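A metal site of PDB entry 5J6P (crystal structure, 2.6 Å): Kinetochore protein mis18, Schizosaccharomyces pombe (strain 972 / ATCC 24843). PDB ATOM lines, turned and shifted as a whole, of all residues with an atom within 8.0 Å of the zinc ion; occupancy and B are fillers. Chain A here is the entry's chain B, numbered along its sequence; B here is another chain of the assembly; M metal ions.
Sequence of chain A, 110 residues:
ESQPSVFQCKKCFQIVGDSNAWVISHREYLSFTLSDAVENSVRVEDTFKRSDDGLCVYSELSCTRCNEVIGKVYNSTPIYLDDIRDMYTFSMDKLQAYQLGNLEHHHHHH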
ATOM      1  N   GLN A   8      35.127  24.635  14.686  1.00  0.00           N
ATOM      2  CA  GLN A   8      34.166  25.712  14.404  1.00  0.00           C
ATOM      3  C   GLN A   8      34.012  26.100  12.947  1.00  0.00           C
ATOM      4  O   GLN A   8      34.971  26.090  12.208  1.00  0.00           O
ATOM      5  CB  GLN A   8      34.619  26.980  15.090  1.00  0.00           C
ATOM      6  CG  GLN A   8      35.067  26.910  16.535  1.00  0.00           C
ATOM      7  CD  GLN A   8      35.813  28.170  16.881  1.00  0.00           C
ATOM      8  OE1 GLN A   8      35.278  29.104  17.516  1.00  0.00           O
ATOM      9  NE2 GLN A   8      37.037  28.250  16.364  1.00  0.00           N
ATOM     10  N   CYS A   9      32.821  26.532  12.568  1.00  0.00           N
ATOM     11  CA  CYS A   9      32.605  27.104  11.240  1.00  0.00           C
ATOM     12  C   CYS A   9      33.414  28.395  11.078  1.00  0.00           C
ATOM     13  O   CYS A   9      33.194  29.373  11.791  1.00  0.00           O
ATOM     14  CB  CYS A   9      31.117  27.367  10.997  1.00  0.00           C
ATOM     15  SG  CYS A   9      30.782  28.671   9.786  1.00  0.00           S
ATOM     16  N   LYS A  10      34.344  28.390  10.128  1.00  0.00           N
ATOM     17  CA  LYS A  10      35.221  29.537   9.872  1.00  0.00           C
ATOM     18  C   LYS A  10      34.518  30.876   9.813  1.00  0.00           C
ATOM     19  O   LYS A  10      35.130  31.921  10.093  1.00  0.00           O
ATOM     20  CB  LYS A  10      35.943  29.362   8.548  1.00  0.00           C
ATOM     21  CG  LYS A  10      37.136  28.404   8.597  1.00  0.00           C
ATOM     22  CD  LYS A  10      38.307  28.981   7.803  1.00  0.00           C
ATOM     23  CE  LYS A  10      39.096  27.960   6.996  1.00  0.00           C
ATOM     24  NZ  LYS A  10      39.494  28.616   5.720  1.00  0.00           N
ATOM     25  N   LYS A  11      33.246  30.849   9.397  1.00  0.00           N
ATOM     26  CA  LYS A  11      32.544  32.077   9.094  1.00  0.00           C
ATOM     27  C   LYS A  11      31.969  32.721  10.331  1.00  0.00           C
ATOM     28  O   LYS A  11      32.195  33.878  10.548  1.00  0.00           O
ATOM     29  CB  LYS A  11      31.397  31.785   8.126  1.00  0.00           C
ATOM     30  CG  LYS A  11      31.074  32.995   7.291  1.00  0.00           C
ATOM     31  CD  LYS A  11      29.604  33.206   7.044  1.00  0.00           C
ATOM     32  CE  LYS A  11      29.391  34.602   6.440  1.00  0.00           C
ATOM     33  NZ  LYS A  11      28.522  34.565   5.251  1.00  0.00           N
ATOM     34  N   CYS A  12      31.264  31.954  11.157  1.00  0.00           N
ATOM     35  CA  CYS A  12      30.636  32.500  12.356  1.00  0.00           C
ATOM     36  C   CYS A  12      31.276  32.046  13.671  1.00  0.00           C
ATOM     37  O   CYS A  12      31.020  32.624  14.732  1.00  0.00           O
ATOM     38  CB  CYS A  12      29.141  32.167  12.371  1.00  0.00           C
ATOM     39  SG  CYS A  12      28.761  30.457  12.819  1.00  0.00           S
ATOM     40  N   PHE A  13      32.114  31.008  13.612  1.00  0.00           N
ATOM     41  CA  PHE A  13      32.756  30.476  14.826  1.00  0.00           C
ATOM     42  C   PHE A  13      31.842  29.606  15.720  1.00  0.00           C
ATOM     43  O   PHE A  13      32.159  29.329  16.869  1.00  0.00           O
ATOM     44  CB  PHE A  13      33.419  31.574  15.670  1.00  0.00           C
ATOM     45  CG  PHE A  13      34.668  32.169  15.088  1.00  0.00           C
ATOM     46  CD1 PHE A  13      35.316  31.672  13.964  1.00  0.00           C
ATOM     47  CD2 PHE A  13      35.258  33.238  15.754  1.00  0.00           C
ATOM     48  CE1 PHE A  13      36.472  32.234  13.493  1.00  0.00           C
ATOM     49  CE2 PHE A  13      36.423  33.798  15.297  1.00  0.00           C
ATOM     50  CZ  PHE A  13      37.029  33.301  14.144  1.00  0.00           C
ATOM     51  N   GLN A  14      30.716  29.171  15.197  1.00  0.00           N
ATOM     52  CA  GLN A  14      29.941  28.226  15.932  1.00  0.00           C
ATOM     53  C   GLN A  14      30.711  26.924  16.078  1.00  0.00           C
ATOM     54  O   GLN A  14      31.237  26.387  15.107  1.00  0.00           O
ATOM     55  CB  GLN A  14      28.618  27.941  15.235  1.00  0.00           C
ATOM     56  CG  GLN A  14      27.786  26.962  16.032  1.00  0.00           C
ATOM     57  CD  GLN A  14      26.390  26.778  15.513  1.00  0.00           C
ATOM     58  OE1 GLN A  14      26.105  26.815  14.285  1.00  0.00           O
ATOM     59  NE2 GLN A  14      25.491  26.524  16.449  1.00  0.00           N
ATOM     60  N   ILE A  15      30.750  26.395  17.293  1.00  0.00           N
ATOM     61  CA  ILE A  15      31.399  25.121  17.527  1.00  0.00           C
ATOM     62  C   ILE A  15      30.447  24.034  17.068  1.00  0.00           C
ATOM     63  O   ILE A  15      29.314  24.021  17.508  1.00  0.00           O
ATOM     64  CB  ILE A  15      31.735  24.889  18.994  1.00  0.00           C
ATOM     65  CG1 ILE A  15      32.929  25.770  19.371  1.00  0.00           C
ATOM     66  CG2 ILE A  15      32.052  23.435  19.281  1.00  0.00           C
ATOM     67  CD1 ILE A  15      33.067  26.009  20.857  1.00  0.00           C
ATOM     68  N   VAL A  16      30.940  23.151  16.196  1.00  0.00           N
ATOM     69  CA  VAL A  16      30.141  22.046  15.653  1.00  0.00           C
ATOM     70  C   VAL A  16      30.494  20.678  16.266  1.00  0.00           C
ATOM     71  O   VAL A  16      29.666  19.762  16.297  1.00  0.00           O
ATOM     72  CB  VAL A  16      30.240  22.012  14.125  1.00  0.00           C
ATOM     73  CG1 VAL A  16      29.804  23.353  13.528  1.00  0.00           C
ATOM     74  CG2 VAL A  16      31.642  21.640  13.657  1.00  0.00           C
ATOM     75  N   SER A  41      23.766  22.641  16.004  1.00  0.00           N
ATOM     76  CA  SER A  41      24.770  23.337  15.202  1.00  0.00           C
ATOM     77  C   SER A  41      24.668  23.153  13.690  1.00  0.00           C
ATOM     78  O   SER A  41      25.331  23.876  12.942  1.00  0.00           O
ATOM     79  CB  SER A  41      26.161  22.921  15.629  1.00  0.00           C
ATOM     80  OG  SER A  41      26.359  21.557  15.358  1.00  0.00           O
ATOM     81  N   SER A  62      24.908  22.124   6.565  1.00  0.00           N
ATOM     82  CA  SER A  62      24.954  23.605   6.730  1.00  0.00           C
ATOM     83  C   SER A  62      25.087  24.052   8.207  1.00  0.00           C
ATOM     84  O   SER A  62      24.517  23.389   9.065  1.00  0.00           O
ATOM     85  CB  SER A  62      23.681  24.174   6.163  1.00  0.00           C
ATOM     86  OG  SER A  62      23.577  23.933   4.758  1.00  0.00           O
ATOM     87  N   CYS A  63      25.792  25.153   8.455  1.00  0.00           N
ATOM     88  CA  CYS A  63      25.890  25.722   9.787  1.00  0.00           C
ATOM     89  C   CYS A  63      24.623  26.511  10.107  1.00  0.00           C
ATOM     90  O   CYS A  63      24.407  27.609   9.572  1.00  0.00           O
ATOM     91  CB  CYS A  63      27.117  26.633   9.894  1.00  0.00           C
ATOM     92  SG  CYS A  63      26.994  27.908  11.164  1.00  0.00           S
ATOM     93  N   THR A  64      23.796  25.961  10.982  1.00  0.00           N
ATOM     94  CA  THR A  64      22.496  26.564  11.349  1.00  0.00           C
ATOM     95  C   THR A  64      22.521  28.047  11.613  1.00  0.00           C
ATOM     96  O   THR A  64      21.510  28.694  11.442  1.00  0.00           O
ATOM     97  CB  THR A  64      21.936  25.998  12.630  1.00  0.00           C
ATOM     98  OG1 THR A  64      23.011  25.888  13.557  1.00  0.00           O
ATOM     99  CG2 THR A  64      21.300  24.654  12.376  1.00  0.00           C
ATOM    100  N   ARG A  65      23.655  28.579  12.065  1.00  0.00           N
ATOM    101  CA  ARG A  65      23.814  30.012  12.225  1.00  0.00           C
ATOM    102  C   ARG A  65      24.153  30.789  10.946  1.00  0.00           C
ATOM    103  O   ARG A  65      23.456  31.739  10.628  1.00  0.00           O
ATOM    104  CB  ARG A  65      24.864  30.308  13.304  1.00  0.00           C
ATOM    105  CG  ARG A  65      25.055  31.788  13.545  1.00  0.00           C
ATOM    106  CD  ARG A  65      25.591  32.120  14.907  1.00  0.00           C
ATOM    107  NE  ARG A  65      24.526  32.003  15.892  1.00  0.00           N
ATOM    108  CZ  ARG A  65      24.567  31.220  16.970  1.00  0.00           C
ATOM    109  NH1 ARG A  65      25.671  30.467  17.280  1.00  0.00           N
ATOM    110  NH2 ARG A  65      23.499  31.209  17.769  1.00  0.00           N
ATOM    111  N   CYS A  66      25.236  30.418  10.266  1.00  0.00           N
ATOM    112  CA  CYS A  66      25.727  31.182   9.133  1.00  0.00           C
ATOM    113  C   CYS A  66      25.317  30.592   7.790  1.00  0.00           C
ATOM    114  O   CYS A  66      25.753  31.063   6.735  1.00  0.00           O
ATOM    115  CB  CYS A  66      27.259  31.312   9.197  1.00  0.00           C
ATOM    116  SG  CYS A  66      28.159  29.933   8.443  1.00  0.00           S
ATOM    117  N   ASN A  67      24.478  29.556   7.824  1.00  0.00           N
ATOM    118  CA  ASN A  67      24.002  28.917   6.559  1.00  0.00           C
ATOM    119  C   ASN A  67      25.078  28.413   5.576  1.00  0.00           C
ATOM    120  O   ASN A  67      24.753  28.014   4.507  1.00  0.00           O
ATOM    121  CB  ASN A  67      23.066  29.848   5.813  1.00  0.00           C
ATOM    122  CG  ASN A  67      21.864  30.228   6.637  1.00  0.00           C
ATOM    123  OD1 ASN A  67      21.231  29.390   7.264  1.00  0.00           O
ATOM    124  ND2 ASN A  67      21.569  31.515   6.664  1.00  0.00           N
ATOM    125  N   GLU A  68      26.332  28.402   5.950  1.00  0.00           N
ATOM    126  CA  GLU A  68      27.367  27.987   5.071  1.00  0.00           C
ATOM    127  C   GLU A  68      27.337  26.458   4.957  1.00  0.00           C
ATOM    128  O   GLU A  68      27.015  25.732   5.903  1.00  0.00           O
ATOM    129  CB  GLU A  68      28.708  28.445   5.626  1.00  0.00           C
ATOM    130  CG  GLU A  68      29.812  28.512   4.592  1.00  0.00           C
ATOM    131  CD  GLU A  68      29.775  29.770   3.746  1.00  0.00           C
ATOM    132  OE1 GLU A  68      28.690  30.302   3.495  1.00  0.00           O
ATOM    133  OE2 GLU A  68      30.841  30.232   3.319  1.00  0.00           O
ATOM    134  N   VAL A  69      27.642  25.977   3.765  1.00  0.00           N
ATOM    135  CA  VAL A  69      27.775  24.582   3.509  1.00  0.00           C
ATOM    136  C   VAL A  69      29.195  24.255   3.951  1.00  0.00           C
ATOM    137  O   VAL A  69      30.186  24.811   3.426  1.00  0.00           O
ATOM    138  CB  VAL A  69      27.492  24.230   2.031  1.00  0.00           C
ATOM    139  CG1 VAL A  69      27.810  22.776   1.725  1.00  0.00           C
ATOM    140  CG2 VAL A  69      26.018  24.460   1.727  1.00  0.00           C
ATOM    141  N   ILE A  70      29.262  23.376   4.939  1.00  0.00           N
ATOM    142  CA  ILE A  70      30.497  23.036   5.648  1.00  0.00           C
ATOM    143  C   ILE A  70      30.835  21.560   5.604  1.00  0.00           C
ATOM    144  O   ILE A  70      31.859  21.151   6.116  1.00  0.00           O
ATOM    145  CB  ILE A  70      30.451  23.457   7.165  1.00  0.00           C
ATOM    146  CG1 ILE A  70      29.288  22.792   7.895  1.00  0.00           C
ATOM    147  CG2 ILE A  70      30.363  24.968   7.324  1.00  0.00           C
ATOM    148  CD1 ILE A  70      29.286  23.068   9.373  1.00  0.00           C
ATOM    149  N   LYS A  94      36.423  24.719   5.375  1.00  0.00           N
ATOM    150  CA  LYS A  94      35.287  25.419   5.929  1.00  0.00           C
ATOM    151  C   LYS A  94      35.240  25.356   7.433  1.00  0.00           C
ATOM    152  O   LYS A  94      34.349  25.920   8.008  1.00  0.00           O
ATOM    153  CB  LYS A  94      34.017  24.776   5.346  1.00  0.00           C
ATOM    154  CG  LYS A  94      33.834  24.987   3.828  1.00  0.00           C
ATOM    155  CD  LYS A  94      33.232  26.347   3.606  1.00  0.00           C
ATOM    156  CE  LYS A  94      32.956  26.678   2.158  1.00  0.00           C
ATOM    157  NZ  LYS A  94      32.235  27.979   2.145  1.00  0.00           N
ATOM    158  N   ARG B  65      37.231  40.476  17.938  1.00  0.00           N
ATOM    159  CA  ARG B  65      36.298  40.355  16.829  1.00  0.00           C
ATOM    160  C   ARG B  65      35.100  41.267  17.018  1.00  0.00           C
ATOM    161  O   ARG B  65      34.768  41.965  16.091  1.00  0.00           O
ATOM    162  CB  ARG B  65      35.825  38.890  16.712  1.00  0.00           C
ATOM    163  CG  ARG B  65      34.867  38.639  15.566  1.00  0.00           C
ATOM    164  CD  ARG B  65      34.968  37.197  15.140  1.00  0.00           C
ATOM    165  NE  ARG B  65      33.757  36.702  14.489  1.00  0.00           N
ATOM    166  CZ  ARG B  65      33.685  36.150  13.279  1.00  0.00           C
ATOM    167  NH1 ARG B  65      34.760  35.987  12.512  1.00  0.00           N
ATOM    168  NH2 ARG B  65      32.488  35.739  12.834  1.00  0.00           N
HETATM  169 ZN    ZN M   1      28.637  29.213  10.426  1.00  0.00          ZN
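The side-chain sulfur of Cys 66 lies close to the backbone NH of Glu 68 (3.4 Å).
SG of Cys 63 lies close to N of Arg 65 of chain A.
N of Cys 63 sits at hydrogen-bond distance from O of Glu 68, at 2.9 Å.
SG of Cys 63 sits close to OE1 of Gln 14 (3.4 Å).
The side-chain sulfur of Cys 9 sits close to the backbone NH of Lys 11, 3.3 Å away.
The backbone NH (N) of Cys 9 is in hydrogen-bond range of the backbone carbonyl oxygen (O) of Gln 14 (3.0 Å).
SG of Cys 12 lies close to N of Gln 14 (3.3 Å).
The zinc ion is bound by SG of Cys 66 (2.2 Å), SG of Cys 63 (2.2 Å), SG of Cys 9 (2.3 Å) and SG of Cys 12 (2.7 Å).
Within 4 Å of the zinc ion: Cys 9, Cys 12, Cys 63 and Cys 66.
Along chain A the residues within 4 Å of the zinc ion span positions 9 to 66.
The nearest printed residue that does not touch the zinc ion is Lys 11 (4.4 Å).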
